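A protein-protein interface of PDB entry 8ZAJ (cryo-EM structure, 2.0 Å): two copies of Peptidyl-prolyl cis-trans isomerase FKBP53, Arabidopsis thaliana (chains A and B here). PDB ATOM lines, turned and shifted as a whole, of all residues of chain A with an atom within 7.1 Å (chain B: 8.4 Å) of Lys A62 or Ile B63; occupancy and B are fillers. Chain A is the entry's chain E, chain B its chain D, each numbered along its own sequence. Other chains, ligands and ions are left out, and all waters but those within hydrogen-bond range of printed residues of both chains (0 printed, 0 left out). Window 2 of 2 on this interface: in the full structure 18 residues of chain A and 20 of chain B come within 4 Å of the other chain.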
ATOM      1  N   LYS A  38       4.913 -10.067   0.160  1.00  0.00           N
ATOM      2  CA  LYS A  38       4.545 -11.248   0.927  1.00  0.00           C
ATOM      3  C   LYS A  38       5.716 -11.862   1.684  1.00  0.00           C
ATOM      4  O   LYS A  38       5.507 -12.806   2.452  1.00  0.00           O
ATOM      5  CB  LYS A  38       3.939 -12.313   0.004  1.00  0.00           C
ATOM      6  CG  LYS A  38       2.629 -11.924  -0.675  1.00  0.00           C
ATOM      7  CD  LYS A  38       1.793 -10.982   0.175  1.00  0.00           C
ATOM      8  CE  LYS A  38       0.701 -10.322  -0.651  1.00  0.00           C
ATOM      9  NZ  LYS A  38       1.240  -9.244  -1.524  1.00  0.00           N
ATOM     10  N   LEU A  58       8.114 -11.871  11.340  1.00  0.00           N
ATOM     11  CA  LEU A  58       6.721 -11.541  11.082  1.00  0.00           C
ATOM     12  C   LEU A  58       6.355 -11.984   9.675  1.00  0.00           C
ATOM     13  O   LEU A  58       7.093 -11.713   8.723  1.00  0.00           O
ATOM     14  CB  LEU A  58       6.472 -10.042  11.250  1.00  0.00           C
ATOM     15  CG  LEU A  58       6.372  -9.553  12.694  1.00  0.00           C
ATOM     16  CD1 LEU A  58       6.097  -8.064  12.736  1.00  0.00           C
ATOM     17  CD2 LEU A  58       5.294 -10.320  13.437  1.00  0.00           C
ATOM     18  N   LEU A  59       5.220 -12.665   9.551  1.00  0.00           N
ATOM     19  CA  LEU A  59       4.748 -13.157   8.267  1.00  0.00           C
ATOM     20  C   LEU A  59       3.600 -12.288   7.783  1.00  0.00           C
ATOM     21  O   LEU A  59       2.554 -12.236   8.446  1.00  0.00           O
ATOM     22  CB  LEU A  59       4.304 -14.613   8.381  1.00  0.00           C
ATOM     23  CG  LEU A  59       5.311 -15.671   7.928  1.00  0.00           C
ATOM     24  CD1 LEU A  59       5.781 -15.389   6.510  1.00  0.00           C
ATOM     25  CD2 LEU A  59       6.491 -15.739   8.884  1.00  0.00           C
ATOM     26  N   PRO A  60       3.749 -11.580   6.665  1.00  0.00           N
ATOM     27  CA  PRO A  60       2.625 -10.801   6.133  1.00  0.00           C
ATOM     28  C   PRO A  60       1.422 -11.687   5.851  1.00  0.00           C
ATOM     29  O   PRO A  60       1.551 -12.794   5.324  1.00  0.00           O
ATOM     30  CB  PRO A  60       3.194 -10.198   4.844  1.00  0.00           C
ATOM     31  CG  PRO A  60       4.663 -10.157   5.066  1.00  0.00           C
ATOM     32  CD  PRO A  60       4.989 -11.359   5.902  1.00  0.00           C
ATOM     33  N   ASN A  61       0.243 -11.187   6.223  1.00  0.00           N
ATOM     34  CA  ASN A  61      -1.060 -11.822   6.055  1.00  0.00           C
ATOM     35  C   ASN A  61      -1.234 -13.071   6.911  1.00  0.00           C
ATOM     36  O   ASN A  61      -2.320 -13.659   6.903  1.00  0.00           O
ATOM     37  CB  ASN A  61      -1.355 -12.180   4.591  1.00  0.00           C
ATOM     38  CG  ASN A  61      -0.993 -11.064   3.635  1.00  0.00           C
ATOM     39  OD1 ASN A  61      -0.119 -11.219   2.783  1.00  0.00           O
ATOM     40  ND2 ASN A  61      -1.663  -9.927   3.774  1.00  0.00           N
ATOM     41  N   LYS A  62      -0.206 -13.503   7.642  1.00  0.00           N
ATOM     42  CA  LYS A  62      -0.329 -14.631   8.558  1.00  0.00           C
ATOM     43  C   LYS A  62      -0.110 -14.208  10.003  1.00  0.00           C
ATOM     44  O   LYS A  62      -0.993 -14.412  10.842  1.00  0.00           O
ATOM     45  CB  LYS A  62       0.662 -15.736   8.168  1.00  0.00           C
ATOM     46  CG  LYS A  62       0.302 -16.479   6.896  1.00  0.00           C
ATOM     47  CD  LYS A  62       1.400 -17.454   6.510  1.00  0.00           C
ATOM     48  CE  LYS A  62       0.975 -18.341   5.354  1.00  0.00           C
ATOM     49  NZ  LYS A  62       2.105 -18.612   4.424  1.00  0.00           N
ATOM     50  N   ILE A  63       1.043 -13.625  10.319  1.00  0.00           N
ATOM     51  CA  ILE A  63       1.336 -13.101  11.653  1.00  0.00           C
ATOM     52  C   ILE A  63       1.925 -11.710  11.440  1.00  0.00           C
ATOM     53  O   ILE A  63       3.130 -11.556  11.220  1.00  0.00           O
ATOM     54  CB  ILE A  63       2.296 -13.995  12.447  1.00  0.00           C
ATOM     55  CG1 ILE A  63       1.908 -15.470  12.307  1.00  0.00           C
ATOM     56  CG2 ILE A  63       2.326 -13.577  13.908  1.00  0.00           C
ATOM     57  CD1 ILE A  63       2.442 -16.357  13.411  1.00  0.00           C
ATOM     58  N   GLU A  64       1.078 -10.686  11.500  1.00  0.00           N
ATOM     59  CA  GLU A  64       1.524  -9.317  11.289  1.00  0.00           C
ATOM     60  C   GLU A  64       1.913  -8.616  12.581  1.00  0.00           C
ATOM     61  O   GLU A  64       2.383  -7.475  12.531  1.00  0.00           O
ATOM     62  CB  GLU A  64       0.441  -8.511  10.571  1.00  0.00           C
ATOM     63  CG  GLU A  64      -0.052  -9.151   9.286  1.00  0.00           C
ATOM     64  CD  GLU A  64       0.070  -8.228   8.090  1.00  0.00           C
ATOM     65  OE1 GLU A  64       0.298  -7.018   8.292  1.00  0.00           O
ATOM     66  OE2 GLU A  64      -0.063  -8.714   6.949  1.00  0.00           O
ATOM     67  N   CYS A  65       1.728  -9.263  13.726  1.00  0.00           N
ATOM     68  CA  CYS A  65       2.191  -8.738  14.998  1.00  0.00           C
ATOM     69  C   CYS A  65       2.572  -9.904  15.894  1.00  0.00           C
ATOM     70  O   CYS A  65       2.031 -11.004  15.767  1.00  0.00           O
ATOM     71  CB  CYS A  65       1.130  -7.866  15.682  1.00  0.00           C
ATOM     72  SG  CYS A  65      -0.333  -8.760  16.249  1.00  0.00           S
ATOM     73  N   GLN B  29      -4.760  -6.797  25.707  1.00  0.00           N
ATOM     74  CA  GLN B  29      -5.385  -7.565  24.643  1.00  0.00           C
ATOM     75  C   GLN B  29      -6.116  -6.623  23.701  1.00  0.00           C
ATOM     76  O   GLN B  29      -6.708  -5.634  24.136  1.00  0.00           O
ATOM     77  CB  GLN B  29      -6.357  -8.608  25.206  1.00  0.00           C
ATOM     78  CG  GLN B  29      -6.776  -9.667  24.206  1.00  0.00           C
ATOM     79  CD  GLN B  29      -5.850 -10.864  24.208  1.00  0.00           C
ATOM     80  OE1 GLN B  29      -5.898 -11.702  23.309  1.00  0.00           O
ATOM     81  NE2 GLN B  29      -5.000 -10.950  25.223  1.00  0.00           N
ATOM     82  N   ALA B  30      -6.063  -6.941  22.412  1.00  0.00           N
ATOM     83  CA  ALA B  30      -6.872  -6.287  21.395  1.00  0.00           C
ATOM     84  C   ALA B  30      -7.685  -7.362  20.693  1.00  0.00           C
ATOM     85  O   ALA B  30      -7.117  -8.291  20.111  1.00  0.00           O
ATOM     86  CB  ALA B  30      -6.005  -5.524  20.393  1.00  0.00           C
ATOM     87  N   THR B  31      -9.007  -7.238  20.749  1.00  0.00           N
ATOM     88  CA  THR B  31      -9.909  -8.233  20.191  1.00  0.00           C
ATOM     89  C   THR B  31     -10.733  -7.598  19.083  1.00  0.00           C
ATOM     90  O   THR B  31     -11.287  -6.509  19.260  1.00  0.00           O
ATOM     91  CB  THR B  31     -10.829  -8.815  21.268  1.00  0.00           C
ATOM     92  OG1 THR B  31     -10.076  -9.063  22.461  1.00  0.00           O
ATOM     93  CG2 THR B  31     -11.454 -10.114  20.788  1.00  0.00           C
ATOM     94  N   LEU B  32     -10.805  -8.277  17.944  1.00  0.00           N
ATOM     95  CA  LEU B  32     -11.608  -7.790  16.835  1.00  0.00           C
ATOM     96  C   LEU B  32     -13.086  -7.816  17.196  1.00  0.00           C
ATOM     97  O   LEU B  32     -13.590  -8.792  17.755  1.00  0.00           O
ATOM     98  CB  LEU B  32     -11.357  -8.636  15.590  1.00  0.00           C
ATOM     99  CG  LEU B  32     -11.189  -7.885  14.271  1.00  0.00           C
ATOM    100  CD1 LEU B  32     -10.383  -6.615  14.478  1.00  0.00           C
ATOM    101  CD2 LEU B  32     -10.528  -8.779  13.238  1.00  0.00           C
ATOM    102  N   LYS B  40      -7.461  -6.695   6.819  1.00  0.00           N
ATOM    103  CA  LYS B  40      -6.655  -6.607   8.028  1.00  0.00           C
ATOM    104  C   LYS B  40      -6.917  -5.295   8.759  1.00  0.00           C
ATOM    105  O   LYS B  40      -7.023  -4.231   8.145  1.00  0.00           O
ATOM    106  CB  LYS B  40      -5.178  -6.754   7.661  1.00  0.00           C
ATOM    107  CG  LYS B  40      -4.199  -5.875   8.412  1.00  0.00           C
ATOM    108  CD  LYS B  40      -2.966  -5.651   7.541  1.00  0.00           C
ATOM    109  CE  LYS B  40      -2.016  -4.629   8.131  1.00  0.00           C
ATOM    110  NZ  LYS B  40      -1.143  -4.015   7.095  1.00  0.00           N
ATOM    111  N   SER B  41      -7.032  -5.379  10.083  1.00  0.00           N
ATOM    112  CA  SER B  41      -7.390  -4.246  10.924  1.00  0.00           C
ATOM    113  C   SER B  41      -6.213  -3.871  11.813  1.00  0.00           C
ATOM    114  O   SER B  41      -5.628  -4.737  12.473  1.00  0.00           O
ATOM    115  CB  SER B  41      -8.616  -4.567  11.782  1.00  0.00           C
ATOM    116  OG  SER B  41      -9.680  -5.061  10.987  1.00  0.00           O
ATOM    117  N   CYS B  56      -0.876  -2.982  16.886  1.00  0.00           N
ATOM    118  CA  CYS B  56      -1.029  -4.389  16.552  1.00  0.00           C
ATOM    119  C   CYS B  56      -1.809  -4.495  15.254  1.00  0.00           C
ATOM    120  O   CYS B  56      -2.482  -3.552  14.833  1.00  0.00           O
ATOM    121  CB  CYS B  56      -1.738  -5.160  17.668  1.00  0.00           C
ATOM    122  SG  CYS B  56      -3.525  -4.914  17.715  1.00  0.00           S
ATOM    123  N   SER B  57      -1.708  -5.659  14.625  1.00  0.00           N
ATOM    124  CA  SER B  57      -2.448  -5.962  13.410  1.00  0.00           C
ATOM    125  C   SER B  57      -3.248  -7.236  13.630  1.00  0.00           C
ATOM    126  O   SER B  57      -2.690  -8.259  14.038  1.00  0.00           O
ATOM    127  CB  SER B  57      -1.510  -6.115  12.213  1.00  0.00           C
ATOM    128  OG  SER B  57      -2.240  -6.225  11.006  1.00  0.00           O
ATOM    129  N   LEU B  58      -4.548  -7.169  13.362  1.00  0.00           N
ATOM    130  CA  LEU B  58      -5.458  -8.280  13.585  1.00  0.00           C
ATOM    131  C   LEU B  58      -6.025  -8.738  12.253  1.00  0.00           C
ATOM    132  O   LEU B  58      -6.468  -7.915  11.447  1.00  0.00           O
ATOM    133  CB  LEU B  58      -6.588  -7.883  14.537  1.00  0.00           C
ATOM    134  CG  LEU B  58      -6.209  -7.830  16.016  1.00  0.00           C
ATOM    135  CD1 LEU B  58      -7.410  -7.455  16.861  1.00  0.00           C
ATOM    136  CD2 LEU B  58      -5.633  -9.161  16.461  1.00  0.00           C
ATOM    137  N   LEU B  59      -6.005 -10.048  12.026  1.00  0.00           N
ATOM    138  CA  LEU B  59      -6.508 -10.627  10.791  1.00  0.00           C
ATOM    139  C   LEU B  59      -7.855 -11.281  11.050  1.00  0.00           C
ATOM    140  O   LEU B  59      -7.926 -12.236  11.838  1.00  0.00           O
ATOM    141  CB  LEU B  59      -5.518 -11.648  10.235  1.00  0.00           C
ATOM    142  CG  LEU B  59      -4.591 -11.161   9.120  1.00  0.00           C
ATOM    143  CD1 LEU B  59      -5.396 -10.556   7.981  1.00  0.00           C
ATOM    144  CD2 LEU B  59      -3.579 -10.161   9.657  1.00  0.00           C
ATOM    145  N   PRO B  60      -8.938 -10.800  10.442  1.00  0.00           N
ATOM    146  CA  PRO B  60     -10.233 -11.467  10.611  1.00  0.00           C
ATOM    147  C   PRO B  60     -10.171 -12.919  10.161  1.00  0.00           C
ATOM    148  O   PRO B  60      -9.576 -13.245   9.132  1.00  0.00           O
ATOM    149  CB  PRO B  60     -11.173 -10.643   9.726  1.00  0.00           C
ATOM    150  CG  PRO B  60     -10.532  -9.305   9.644  1.00  0.00           C
ATOM    151  CD  PRO B  60      -9.052  -9.551   9.672  1.00  0.00           C
ATOM    152  N   ASN B  61     -10.787 -13.792  10.958  1.00  0.00           N
ATOM    153  CA  ASN B  61     -10.889 -15.233  10.749  1.00  0.00           C
ATOM    154  C   ASN B  61      -9.551 -15.953  10.868  1.00  0.00           C
ATOM    155  O   ASN B  61      -9.521 -17.185  10.776  1.00  0.00           O
ATOM    156  CB  ASN B  61     -11.524 -15.589   9.397  1.00  0.00           C
ATOM    157  CG  ASN B  61     -12.747 -14.750   9.090  1.00  0.00           C
ATOM    158  OD1 ASN B  61     -12.765 -13.986   8.126  1.00  0.00           O
ATOM    159  ND2 ASN B  61     -13.778 -14.883   9.916  1.00  0.00           N
ATOM    160  N   LYS B  62      -8.445 -15.235  11.062  1.00  0.00           N
ATOM    161  CA  LYS B  62      -7.145 -15.861  11.281  1.00  0.00           C
ATOM    162  C   LYS B  62      -6.600 -15.547  12.666  1.00  0.00           C
ATOM    163  O   LYS B  62      -6.321 -16.468  13.439  1.00  0.00           O
ATOM    164  CB  LYS B  62      -6.156 -15.411  10.200  1.00  0.00           C
ATOM    165  CG  LYS B  62      -6.421 -15.995   8.825  1.00  0.00           C
ATOM    166  CD  LYS B  62      -5.485 -15.394   7.791  1.00  0.00           C
ATOM    167  CE  LYS B  62      -5.606 -16.103   6.455  1.00  0.00           C
ATOM    168  NZ  LYS B  62      -5.481 -15.153   5.315  1.00  0.00           N
ATOM    169  N   ILE B  63      -6.434 -14.270  13.001  1.00  0.00           N
ATOM    170  CA  ILE B  63      -5.994 -13.841  14.329  1.00  0.00           C
ATOM    171  C   ILE B  63      -6.934 -12.713  14.741  1.00  0.00           C
ATOM    172  O   ILE B  63      -6.718 -11.546  14.398  1.00  0.00           O
ATOM    173  CB  ILE B  63      -4.532 -13.383  14.353  1.00  0.00           C
ATOM    174  CG1 ILE B  63      -3.644 -14.347  13.563  1.00  0.00           C
ATOM    175  CG2 ILE B  63      -4.042 -13.241  15.785  1.00  0.00           C
ATOM    176  CD1 ILE B  63      -2.178 -14.284  13.935  1.00  0.00           C
ATOM    177  N   GLU B  64      -7.989 -13.053  15.476  1.00  0.00           N
ATOM    178  CA  GLU B  64      -8.966 -12.062  15.906  1.00  0.00           C
ATOM    179  C   GLU B  64      -8.647 -11.471  17.270  1.00  0.00           C
ATOM    180  O   GLU B  64      -9.356 -10.563  17.716  1.00  0.00           O
ATOM    181  CB  GLU B  64     -10.367 -12.675  15.925  1.00  0.00           C
ATOM    182  CG  GLU B  64     -10.769 -13.335  14.619  1.00  0.00           C
ATOM    183  CD  GLU B  64     -12.065 -12.784  14.061  1.00  0.00           C
ATOM    184  OE1 GLU B  64     -12.781 -12.077  14.799  1.00  0.00           O
ATOM    185  OE2 GLU B  64     -12.368 -13.061  12.881  1.00  0.00           O
ATOM    186  N   CYS B  65      -7.610 -11.960  17.939  1.00  0.00           N
ATOM    187  CA  CYS B  65      -7.140 -11.373  19.182  1.00  0.00           C
ATOM    188  C   CYS B  65      -5.635 -11.557  19.267  1.00  0.00           C
ATOM    189  O   CYS B  65      -5.079 -12.506  18.709  1.00  0.00           O
ATOM    190  CB  CYS B  65      -7.824 -11.998  20.406  1.00  0.00           C
ATOM    191  SG  CYS B  65      -7.392 -13.724  20.715  1.00  0.00           S
ATOM    192  N   CYS B  66      -4.975 -10.640  19.971  1.00  0.00           N
ATOM    193  CA  CYS B  66      -3.538 -10.718  20.109  1.00  0.00           C
ATOM    194  C   CYS B  66      -3.142 -10.130  21.451  1.00  0.00           C
ATOM    195  O   CYS B  66      -3.694  -9.096  21.853  1.00  0.00           O
ATOM    196  CB  CYS B  66      -2.810  -9.981  18.981  1.00  0.00           C
ATOM    197  SG  CYS B  66      -3.171  -8.219  18.879  1.00  0.00           S
ATOM    198  N   PRO B  67      -2.217 -10.761  22.166  1.00  0.00           N
ATOM    199  CA  PRO B  67      -1.759 -10.194  23.434  1.00  0.00           C
ATOM    200  C   PRO B  67      -1.007  -8.893  23.218  1.00  0.00           C
ATOM    201  O   PRO B  67      -0.331  -8.695  22.205  1.00  0.00           O
ATOM    202  CB  PRO B  67      -0.841 -11.282  24.000  1.00  0.00           C
ATOM    203  CG  PRO B  67      -0.385 -12.040  22.807  1.00  0.00           C
ATOM    204  CD  PRO B  67      -1.526 -12.018  21.837  1.00  0.00           C
ATOM    205  N   ARG B  87     -14.211  -2.686  11.320  1.00  0.00           N
ATOM    206  CA  ARG B  87     -14.505  -3.440  12.531  1.00  0.00           C
ATOM    207  C   ARG B  87     -13.917  -2.715  13.732  1.00  0.00           C
ATOM    208  O   ARG B  87     -12.765  -2.272  13.692  1.00  0.00           O
ATOM    209  CB  ARG B  87     -13.946  -4.861  12.455  1.00  0.00           C
ATOM    210  CG  ARG B  87     -14.678  -5.779  11.495  1.00  0.00           C
ATOM    211  CD  ARG B  87     -13.699  -6.682  10.765  1.00  0.00           C
ATOM    212  NE  ARG B  87     -14.311  -7.937  10.342  1.00  0.00           N
ATOM    213  CZ  ARG B  87     -14.583  -8.950  11.152  1.00  0.00           C
ATOM    214  NH1 ARG B  87     -14.319  -8.893  12.447  1.00  0.00           N
ATOM    215  NH2 ARG B  87     -15.134 -10.052  10.650  1.00  0.00           N
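O of Ala B30 sits at hydrogen-bond distance from N of Cys B66.
SG of Cys B56 sits at hydrogen-bond distance from SG of Cys B66, 3.5 Å away.
The side-chain carboxylate of Glu A64 is in hydrogen-bond range of the backbone NH of Asn A61, 2.6 Å away.
OE1 of Glu A64 lies within salt-bridge range of NZ of Lys B40 (3.5 Å).
The backbone carbonyl oxygen (O) of Ser B57 is in hydrogen-bond range of the side-chain sulfur (SG) of Cys A65 (3.3 Å).
Leu A59 touches none of the printed residues of chain B.
Of the printed residues of chain B, Asn A61 touches Lys B62 (3.7 Å).
Of the printed residues of chain B, Glu A64 touches Lys B40 (3.3 Å), Ser B57 (3.5 Å) and Leu B59 (3.7 Å).
Thr B31 touches none of the printed residues of chain A.
Of the printed residues of chain A, Lys B40 touches Glu A64 (3.3 Å).
Of the printed residues of chain A, Ser B57 touches Glu A64 (3.5 Å) and Cys A65 (3.3 Å).
The nearest residue of chain A that does not touch Ile B63 is Ile A63 (4.4 Å).
The nearest printed residue of chain A that does not touch Lys B40 is Asn A61 (5.8 Å).
Asn A61 touches Lys B62.
Lys A62 touches Ile B63.
Ser B57 touches Glu A64 (CB to CB, 3.5 Å).
Leu B59 touches Glu A64.
Cys A65 touches Cys B66.
Asn A61 touches Lys B62, but with the chains exchanged Lys A62 does not touch Asn B61 (8.7 Å).
Lys A62 touches Ile B63, but with the chains exchanged Ile A63 does not touch Lys B62 (7.2 Å).
Glu A64 touches Leu B59, but with the chains exchanged Leu A59 does not touch Glu B64 (12.7 Å).
Positions printed for both chains: 58, 59, 60, 61, 62, 63, 64 and 65.
Of the 7 pairs that touch across the chains among the printed residues, none has its exchanged pair printed and touching as well.
Printed residues of chain B that touch a printed residue of chain A: Lys B40, Ser B57, Leu B59, Lys B62, Ile B63 and Cys B66.
Hydrophobic or aromatic side chains of chain B that line the printed part of chain A: Leu B59 and Ile B63.
Along chain B the printed residues that touch a printed residue of chain A span positions 40 to 66.
Of the 9 printed residues of chain A, 4 touch a printed residue of chain B.
Along chain A the printed residues that touch a printed residue of chain B span positions 61 to 65.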
